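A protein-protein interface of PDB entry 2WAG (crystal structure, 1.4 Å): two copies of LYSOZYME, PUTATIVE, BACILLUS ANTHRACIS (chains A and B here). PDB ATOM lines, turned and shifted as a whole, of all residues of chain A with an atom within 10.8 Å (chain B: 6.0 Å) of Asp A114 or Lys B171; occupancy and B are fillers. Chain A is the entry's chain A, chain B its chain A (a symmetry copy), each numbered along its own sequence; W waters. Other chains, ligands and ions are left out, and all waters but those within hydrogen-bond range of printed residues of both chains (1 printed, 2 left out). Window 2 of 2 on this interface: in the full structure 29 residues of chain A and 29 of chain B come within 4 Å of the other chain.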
ATOM      1  N   PHE A  78     -24.375  -6.260 -31.407  1.00  0.00           N
ATOM      2  CA  PHE A  78     -25.526  -5.933 -32.244  1.00  0.00           C
ATOM      3  C   PHE A  78     -25.156  -5.771 -33.714  1.00  0.00           C
ATOM      4  O   PHE A  78     -26.036  -5.522 -34.536  1.00  0.00           O
ATOM      5  CB  PHE A  78     -26.192  -4.663 -31.712  1.00  0.00           C
ATOM      6  CG  PHE A  78     -26.742  -4.827 -30.329  1.00  0.00           C
ATOM      7  CD1 PHE A  78     -27.847  -5.615 -30.105  1.00  0.00           C
ATOM      8  CD2 PHE A  78     -26.145  -4.199 -29.239  1.00  0.00           C
ATOM      9  CE1 PHE A  78     -28.375  -5.794 -28.821  1.00  0.00           C
ATOM     10  CE2 PHE A  78     -26.670  -4.376 -27.958  1.00  0.00           C
ATOM     11  CZ  PHE A  78     -27.778  -5.161 -27.751  1.00  0.00           C
ATOM     12  N   GLU A 107     -26.415  -6.669 -23.506  1.00  0.00           N
ATOM     13  CA  GLU A 107     -26.557  -5.399 -22.778  1.00  0.00           C
ATOM     14  C   GLU A 107     -26.040  -4.273 -23.651  1.00  0.00           C
ATOM     15  O   GLU A 107     -25.353  -4.506 -24.649  1.00  0.00           O
ATOM     16  CB  GLU A 107     -25.810  -5.414 -21.435  1.00  0.00           C
ATOM     17  CG  GLU A 107     -24.313  -5.531 -21.544  1.00  0.00           C
ATOM     18  CD  GLU A 107     -23.695  -5.699 -20.177  1.00  0.00           C
ATOM     19  OE1 GLU A 107     -23.619  -4.692 -19.424  1.00  0.00           O
ATOM     20  OE2 GLU A 107     -23.299  -6.832 -19.823  1.00  0.00           O
ATOM     21  N   PHE A 108     -26.363  -3.045 -23.267  1.00  0.00           N
ATOM     22  CA  PHE A 108     -25.845  -1.916 -24.023  1.00  0.00           C
ATOM     23  C   PHE A 108     -24.360  -1.658 -23.786  1.00  0.00           C
ATOM     24  O   PHE A 108     -23.827  -1.940 -22.708  1.00  0.00           O
ATOM     25  CB  PHE A 108     -26.663  -0.663 -23.761  1.00  0.00           C
ATOM     26  CG  PHE A 108     -28.048  -0.759 -24.300  1.00  0.00           C
ATOM     27  CD1 PHE A 108     -28.244  -0.775 -25.670  1.00  0.00           C
ATOM     28  CD2 PHE A 108     -29.141  -0.870 -23.469  1.00  0.00           C
ATOM     29  CE1 PHE A 108     -29.504  -0.891 -26.205  1.00  0.00           C
ATOM     30  CE2 PHE A 108     -30.430  -0.993 -24.008  1.00  0.00           C
ATOM     31  CZ  PHE A 108     -30.599  -0.990 -25.390  1.00  0.00           C
ATOM     32  N   TYR A 109     -23.713  -1.122 -24.816  1.00  0.00           N
ATOM     33  CA  TYR A 109     -22.301  -0.781 -24.777  1.00  0.00           C
ATOM     34  C   TYR A 109     -22.048   0.312 -25.808  1.00  0.00           C
ATOM     35  O   TYR A 109     -22.936   0.649 -26.591  1.00  0.00           O
ATOM     36  CB  TYR A 109     -21.446  -2.009 -25.091  1.00  0.00           C
ATOM     37  CG  TYR A 109     -21.727  -2.618 -26.446  1.00  0.00           C
ATOM     38  CD1 TYR A 109     -20.995  -2.241 -27.565  1.00  0.00           C
ATOM     39  CD2 TYR A 109     -22.726  -3.569 -26.608  1.00  0.00           C
ATOM     40  CE1 TYR A 109     -21.250  -2.796 -28.805  1.00  0.00           C
ATOM     41  CE2 TYR A 109     -22.987  -4.129 -27.845  1.00  0.00           C
ATOM     42  CZ  TYR A 109     -22.247  -3.739 -28.939  1.00  0.00           C
ATOM     43  OH  TYR A 109     -22.506  -4.294 -30.171  1.00  0.00           O
ATOM     44  N   ALA A 110     -20.841   0.864 -25.809  1.00  0.00           N
ATOM     45  CA  ALA A 110     -20.496   1.922 -26.751  1.00  0.00           C
ATOM     46  C   ALA A 110     -21.612   2.961 -26.844  1.00  0.00           C
ATOM     47  O   ALA A 110     -22.029   3.527 -25.834  1.00  0.00           O
ATOM     48  CB  ALA A 110     -20.198   1.335 -28.121  1.00  0.00           C
ATOM     49  N   ASN A 111     -22.091   3.207 -28.060  1.00  0.00           N
ATOM     50  CA  ASN A 111     -23.135   4.204 -28.286  1.00  0.00           C
ATOM     51  C   ASN A 111     -24.498   3.590 -28.594  1.00  0.00           C
ATOM     52  O   ASN A 111     -25.425   4.288 -29.004  1.00  0.00           O
ATOM     53  CB  ASN A 111     -22.727   5.158 -29.410  1.00  0.00           C
ATOM     54  CG  ASN A 111     -21.500   5.979 -29.063  1.00  0.00           C
ATOM     55  OD1 ASN A 111     -20.614   6.173 -29.895  1.00  0.00           O
ATOM     56  ND2 ASN A 111     -21.445   6.469 -27.829  1.00  0.00           N
ATOM     57  N   LYS A 112     -24.612   2.275 -28.426  1.00  0.00           N
ATOM     58  CA  LYS A 112     -25.756   1.542 -28.962  1.00  0.00           C
ATOM     59  C   LYS A 112     -27.087   1.971 -28.341  1.00  0.00           C
ATOM     60  O   LYS A 112     -28.144   1.874 -28.971  1.00  0.00           O
ATOM     61  CB  LYS A 112     -25.545   0.026 -28.839  1.00  0.00           C
ATOM     62  CG  LYS A 112     -24.242  -0.488 -29.454  1.00  0.00           C
ATOM     63  CD  LYS A 112     -24.234  -0.478 -30.983  1.00  0.00           C
ATOM     64  CE  LYS A 112     -25.560  -0.879 -31.614  1.00  0.00           C
ATOM     65  NZ  LYS A 112     -25.456  -0.844 -33.096  1.00  0.00           N
ATOM     66  N   LYS A 113     -27.061   2.467 -27.106  1.00  0.00           N
ATOM     67  CA  LYS A 113     -28.291   2.888 -26.473  1.00  0.00           C
ATOM     68  C   LYS A 113     -28.835   4.217 -27.039  1.00  0.00           C
ATOM     69  O   LYS A 113     -30.007   4.517 -26.859  1.00  0.00           O
ATOM     70  CB  LYS A 113     -28.162   2.926 -24.940  1.00  0.00           C
ATOM     71  CG  LYS A 113     -29.495   3.143 -24.236  1.00  0.00           C
ATOM     72  CD  LYS A 113     -29.406   3.120 -22.708  1.00  0.00           C
ATOM     73  CE  LYS A 113     -30.626   3.828 -22.095  1.00  0.00           C
ATOM     74  NZ  LYS A 113     -30.620   3.824 -20.610  1.00  0.00           N
ATOM     75  N   ASP A 114     -28.000   4.990 -27.739  1.00  0.00           N
ATOM     76  CA  ASP A 114     -28.498   6.209 -28.411  1.00  0.00           C
ATOM     77  C   ASP A 114     -29.478   5.872 -29.527  1.00  0.00           C
ATOM     78  O   ASP A 114     -30.314   6.686 -29.893  1.00  0.00           O
ATOM     79  CB  ASP A 114     -27.343   7.027 -29.003  1.00  0.00           C
ATOM     80  CG  ASP A 114     -26.537   7.783 -27.955  1.00  0.00           C
ATOM     81  OD1 ASP A 114     -27.136   8.340 -27.014  1.00  0.00           O
ATOM     82  OD2 ASP A 114     -25.297   7.853 -28.117  1.00  0.00           O
ATOM     83  N   ASN A 115     -29.349   4.678 -30.090  1.00  0.00           N
ATOM     84  CA  ASN A 115     -30.229   4.230 -31.168  1.00  0.00           C
ATOM     85  C   ASN A 115     -30.436   2.733 -31.049  1.00  0.00           C
ATOM     86  O   ASN A 115     -29.809   1.954 -31.773  1.00  0.00           O
ATOM     87  CB  ASN A 115     -29.612   4.568 -32.520  1.00  0.00           C
ATOM     88  CG  ASN A 115     -29.473   6.057 -32.734  1.00  0.00           C
ATOM     89  OD1 ASN A 115     -30.455   6.747 -33.021  1.00  0.00           O
ATOM     90  ND2 ASN A 115     -28.251   6.563 -32.601  1.00  0.00           N
ATOM     91  N   PRO A 116     -31.298   2.325 -30.112  1.00  0.00           N
ATOM     92  CA  PRO A 116     -31.354   0.895 -29.790  1.00  0.00           C
ATOM     93  C   PRO A 116     -31.736   0.031 -30.986  1.00  0.00           C
ATOM     94  O   PRO A 116     -32.651   0.372 -31.759  1.00  0.00           O
ATOM     95  CB  PRO A 116     -32.435   0.815 -28.716  1.00  0.00           C
ATOM     96  CG  PRO A 116     -32.427   2.201 -28.071  1.00  0.00           C
ATOM     97  CD  PRO A 116     -32.120   3.142 -29.200  1.00  0.00           C
ATOM     98  N   PRO A 117     -31.052  -1.094 -31.137  1.00  0.00           N
ATOM     99  CA  PRO A 117     -31.421  -2.056 -32.166  1.00  0.00           C
ATOM    100  C   PRO A 117     -32.870  -2.491 -32.040  1.00  0.00           C
ATOM    101  O   PRO A 117     -33.458  -2.472 -30.948  1.00  0.00           O
ATOM    102  CB  PRO A 117     -30.490  -3.229 -31.869  1.00  0.00           C
ATOM    103  CG  PRO A 117     -29.269  -2.575 -31.316  1.00  0.00           C
ATOM    104  CD  PRO A 117     -29.800  -1.469 -30.448  1.00  0.00           C
ATOM    105  N   LYS A 118     -33.455  -2.887 -33.169  1.00  0.00           N
ATOM    106  CA  LYS A 118     -34.824  -3.348 -33.158  1.00  0.00           C
ATOM    107  C   LYS A 118     -34.913  -4.749 -32.583  1.00  0.00           C
ATOM    108  O   LYS A 118     -34.056  -5.560 -32.833  1.00  0.00           O
ATOM    109  CB  LYS A 118     -35.355  -3.402 -34.578  1.00  0.00           C
ATOM    110  CG  LYS A 118     -35.353  -2.054 -35.231  1.00  0.00           C
ATOM    111  CD  LYS A 118     -36.323  -1.151 -34.512  1.00  0.00           C
ATOM    112  N   GLU A 148     -32.647  -3.011 -18.545  1.00  0.00           N
ATOM    113  CA  GLU A 148     -33.083  -2.334 -19.767  1.00  0.00           C
ATOM    114  C   GLU A 148     -33.024  -3.261 -20.981  1.00  0.00           C
ATOM    115  O   GLU A 148     -33.944  -3.266 -21.813  1.00  0.00           O
ATOM    116  CB  GLU A 148     -32.268  -1.049 -19.985  1.00  0.00           C
ATOM    117  CG  GLU A 148     -32.601   0.017 -18.937  1.00  0.00           C
ATOM    118  CD  GLU A 148     -31.897   1.316 -19.153  1.00  0.00           C
ATOM    119  OE1 GLU A 148     -30.768   1.306 -19.693  1.00  0.00           O
ATOM    120  OE2 GLU A 148     -32.477   2.361 -18.765  1.00  0.00           O
ATOM    121  N   LEU A 152     -36.315  -4.771 -23.173  1.00  0.00           N
ATOM    122  CA  LEU A 152     -36.405  -4.443 -24.593  1.00  0.00           C
ATOM    123  C   LEU A 152     -36.170  -5.614 -25.554  1.00  0.00           C
ATOM    124  O   LEU A 152     -36.555  -5.539 -26.721  1.00  0.00           O
ATOM    125  CB  LEU A 152     -35.444  -3.299 -24.933  1.00  0.00           C
ATOM    126  CG  LEU A 152     -35.906  -1.891 -24.553  1.00  0.00           C
ATOM    127  CD1 LEU A 152     -34.737  -0.917 -24.575  1.00  0.00           C
ATOM    128  CD2 LEU A 152     -37.018  -1.421 -25.478  1.00  0.00           C
ATOM    129  N   TYR A 153     -35.539  -6.696 -25.105  1.00  0.00           N
ATOM    130  CA  TYR A 153     -35.219  -7.776 -25.974  1.00  0.00           C
ATOM    131  C   TYR A 153     -35.571  -9.175 -25.468  1.00  0.00           C
ATOM    132  O   TYR A 153     -35.730 -10.032 -26.238  1.00  0.00           O
ATOM    133  CB  TYR A 153     -33.752  -7.728 -26.313  1.00  0.00           C
ATOM    134  CG  TYR A 153     -33.309  -6.430 -26.934  1.00  0.00           C
ATOM    135  CD1 TYR A 153     -33.934  -5.940 -28.052  1.00  0.00           C
ATOM    136  CD2 TYR A 153     -32.300  -5.696 -26.406  1.00  0.00           C
ATOM    137  CE1 TYR A 153     -33.524  -4.749 -28.619  1.00  0.00           C
ATOM    138  CE2 TYR A 153     -31.903  -4.528 -26.950  1.00  0.00           C
ATOM    139  CZ  TYR A 153     -32.507  -4.065 -28.064  1.00  0.00           C
ATOM    140  OH  TYR A 153     -32.090  -2.867 -28.597  1.00  0.00           O
ATOM    141  N   HIS B   8     -17.378   3.865 -23.888  1.00  0.00           N
ATOM    142  CA  HIS B   8     -18.245   4.993 -24.190  1.00  0.00           C
ATOM    143  C   HIS B   8     -17.345   6.228 -24.139  1.00  0.00           C
ATOM    144  O   HIS B   8     -16.548   6.399 -23.210  1.00  0.00           O
ATOM    145  CB  HIS B   8     -19.347   5.073 -23.132  1.00  0.00           C
ATOM    146  CG  HIS B   8     -20.368   6.138 -23.364  1.00  0.00           C
ATOM    147  ND1 HIS B   8     -21.149   6.237 -24.497  1.00  0.00           N
ATOM    148  CD2 HIS B   8     -20.765   7.140 -22.547  1.00  0.00           C
ATOM    149  CE1 HIS B   8     -21.977   7.261 -24.363  1.00  0.00           C
ATOM    150  NE2 HIS B   8     -21.771   7.815 -23.178  1.00  0.00           N
ATOM    151  N   MET B  11     -18.540  13.252 -26.290  1.00  0.00           N
ATOM    152  CA  MET B  11     -18.731  13.958 -27.560  1.00  0.00           C
ATOM    153  C   MET B  11     -17.531  14.855 -27.815  1.00  0.00           C
ATOM    154  O   MET B  11     -16.955  15.444 -26.895  1.00  0.00           O
ATOM    155  CB  MET B  11     -20.048  14.751 -27.555  1.00  0.00           C
ATOM    156  CG  MET B  11     -21.283  13.853 -27.518  1.00  0.00           C
ATOM    157  SD  MET B  11     -22.779  14.689 -26.922  1.00  0.00           S
ATOM    158  CE  MET B  11     -22.918  16.057 -28.069  1.00  0.00           C
ATOM    159  N   SER B 167     -24.108   9.757 -17.362  1.00  0.00           N
ATOM    160  CA  SER B 167     -24.705   9.200 -18.572  1.00  0.00           C
ATOM    161  C   SER B 167     -23.663   8.360 -19.311  1.00  0.00           C
ATOM    162  O   SER B 167     -22.950   8.876 -20.184  1.00  0.00           O
ATOM    163  CB  SER B 167     -25.245  10.320 -19.454  1.00  0.00           C
ATOM    164  OG  SER B 167     -25.980   9.806 -20.554  1.00  0.00           O
ATOM    165  N   LEU B 169     -24.062   5.456 -21.041  1.00  0.00           N
ATOM    166  CA  LEU B 169     -24.499   4.665 -22.206  1.00  0.00           C
ATOM    167  C   LEU B 169     -25.063   5.510 -23.336  1.00  0.00           C
ATOM    168  O   LEU B 169     -25.277   5.008 -24.441  1.00  0.00           O
ATOM    169  CB  LEU B 169     -25.567   3.641 -21.774  1.00  0.00           C
ATOM    170  CG  LEU B 169     -25.108   2.533 -20.831  1.00  0.00           C
ATOM    171  CD1 LEU B 169     -26.303   1.635 -20.391  1.00  0.00           C
ATOM    172  CD2 LEU B 169     -24.028   1.731 -21.480  1.00  0.00           C
ATOM    173  N   THR B 170     -25.336   6.778 -23.066  1.00  0.00           N
ATOM    174  CA  THR B 170     -25.967   7.625 -24.063  1.00  0.00           C
ATOM    175  C   THR B 170     -25.397   9.028 -23.978  1.00  0.00           C
ATOM    176  O   THR B 170     -24.696   9.389 -23.041  1.00  0.00           O
ATOM    177  CB  THR B 170     -27.486   7.789 -23.818  1.00  0.00           C
ATOM    178  OG1 THR B 170     -27.721   8.489 -22.579  1.00  0.00           O
ATOM    179  CG2 THR B 170     -28.232   6.461 -23.802  1.00  0.00           C
ATOM    180  N   LYS B 171     -25.721   9.827 -24.976  1.00  0.00           N
ATOM    181  CA  LYS B 171     -25.471  11.253 -24.880  1.00  0.00           C
ATOM    182  C   LYS B 171     -26.248  11.829 -23.689  1.00  0.00           C
ATOM    183  O   LYS B 171     -27.286  11.305 -23.282  1.00  0.00           O
ATOM    184  CB  LYS B 171     -25.925  11.927 -26.169  1.00  0.00           C
ATOM    185  CG  LYS B 171     -25.116  11.503 -27.389  1.00  0.00           C
ATOM    186  CD  LYS B 171     -25.534  12.261 -28.649  1.00  0.00           C
ATOM    187  CE  LYS B 171     -24.375  12.319 -29.629  1.00  0.00           C
ATOM    188  NZ  LYS B 171     -23.563  11.071 -29.653  1.00  0.00           N
ATOM    189  N   PRO B 172     -25.728  12.901 -23.099  1.00  0.00           N
ATOM    190  CA  PRO B 172     -26.311  13.408 -21.858  1.00  0.00           C
ATOM    191  C   PRO B 172     -27.551  14.249 -22.078  1.00  0.00           C
ATOM    192  O   PRO B 172     -27.601  15.078 -22.988  1.00  0.00           O
ATOM    193  CB  PRO B 172     -25.193  14.281 -21.290  1.00  0.00           C
ATOM    194  CG  PRO B 172     -24.474  14.801 -22.543  1.00  0.00           C
ATOM    195  CD  PRO B 172     -24.507  13.624 -23.498  1.00  0.00           C
ATOM    196  N   SER B 173     -28.572  14.029 -21.258  1.00  0.00           N
ATOM    197  CA  SER B 173     -29.727  14.932 -21.247  1.00  0.00           C
ATOM    198  C   SER B 173     -30.542  14.755 -19.987  1.00  0.00           C
ATOM    199  O   SER B 173     -30.717  13.646 -19.478  1.00  0.00           O
ATOM    200  CB  SER B 173     -30.638  14.718 -22.455  1.00  0.00           C
ATOM    201  OG  SER B 173     -31.411  13.545 -22.272  1.00  0.00           O
ATOM    202  N   TRP B 183     -20.578  16.134 -17.085  1.00  0.00           N
ATOM    203  CA  TRP B 183     -21.159  14.874 -17.580  1.00  0.00           C
ATOM    204  C   TRP B 183     -20.163  13.746 -17.312  1.00  0.00           C
ATOM    205  O   TRP B 183     -19.035  13.793 -17.797  1.00  0.00           O
ATOM    206  CB  TRP B 183     -21.419  15.017 -19.094  1.00  0.00           C
ATOM    207  CG  TRP B 183     -21.645  13.746 -19.867  1.00  0.00           C
ATOM    208  CD1 TRP B 183     -22.169  12.567 -19.412  1.00  0.00           C
ATOM    209  CD2 TRP B 183     -21.372  13.556 -21.264  1.00  0.00           C
ATOM    210  NE1 TRP B 183     -22.194  11.633 -20.437  1.00  0.00           N
ATOM    211  CE2 TRP B 183     -21.727  12.226 -21.584  1.00  0.00           C
ATOM    212  CE3 TRP B 183     -20.882  14.395 -22.283  1.00  0.00           C
ATOM    213  CZ2 TRP B 183     -21.592  11.707 -22.877  1.00  0.00           C
ATOM    214  CZ3 TRP B 183     -20.751  13.873 -23.574  1.00  0.00           C
ATOM    215  CH2 TRP B 183     -21.105  12.540 -23.849  1.00  0.00           C
HETATM  216  O   HOH W   1     -24.145   8.608 -30.401  1.00  0.00           O
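Of the printed residues of chain B, Phe A108 touches Leu B169.
Of the printed residues of chain B, Ala A110 touches His B8 (3.1 Å) and Leu B169 (3.8 Å).
Of the printed residues of chain B, Lys A113 touches Leu B169 (3.6 Å) and Thr B170 (3.6 Å).
Of the printed residues of chain B, Asp A114 touches Thr B170 (3.3 Å) and Lys B171 (2.9 Å).
Printed residues of chain A within 4 Å of Thr B170: Lys A113 (3.6 Å) and Asp A114 (3.3 Å).
Lys B171 touches one residue of chain A.
No residue of chain A comes within 4 Å of Pro B172.
The nearest residue of chain B that does not touch Asp A114 is Leu B169 (4.3 Å).
The nearest residue of chain A that does not touch Lys B171 is Asn A111 (5.4 Å).
The nearest printed residue of chain B that does not touch Asn A111 is Leu B169 (4.5 Å).
Water W1 lies within hydrogen-bond range of the side-chain amino group of Lys B171 (2.6 Å) and the side-chain carboxylate of Asp A114 (2.7 Å).
No position is printed for both chains.
Of the 9 printed residues of chain B, 4 touch a printed residue of chain A.
Printed residues of chain A that touch a printed residue of chain B: Phe A108, Ala A110, Asn A111, Lys A113 and Asp A114.
Among the printed residues, 8 pairs touch across the chains.
Among the printed residues, Asp or Glu carboxylates within 4 Å of a Lys or Arg side-chain nitrogen of the other chain: Asp A114 with Lys B171 (3.97 Å).
A ring nitrogen (NE2) of His B8 is in hydrogen-bond range of the backbone carbonyl oxygen of Ser B167, at 3.4 Å.
The side-chain carboxylate (OE1) of Glu A148 is in salt-bridge range of the side-chain amino group (NZ) of Lys A113, 2.7 Å away.
The side-chain hydroxyl (OG) of Ser B167 lies within hydrogen-bond range of the backbone carbonyl oxygen (O) of Lys B171 (3.4 Å).
A ring nitrogen (NE2) of His B8 is in hydrogen-bond range of the backbone carbonyl oxygen (O) of Thr B170 (3.3 Å).
The backbone carbonyl oxygen (O) of Thr B170 lies within hydrogen-bond range of the side-chain hydroxyl (OG) of Ser B167 (2.8 Å).
ND1 of His B8 sits at hydrogen-bond distance from ND2 of Asn A111 (3.4 Å).
The side-chain carboxylate of Asp A114 is in salt-bridge range of the side-chain amino group of Lys B171 (3.97 Å).
ND1 of His B8 sits at hydrogen-bond distance from O of Ala A110.
Among the printed residues, pairs that only touch across the chains: Asp A114 with Thr B170, Lys A113 with Thr B170, Lys A113 with Leu B169, Ala A110 with Leu B169 and Phe A108 with Leu B169.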
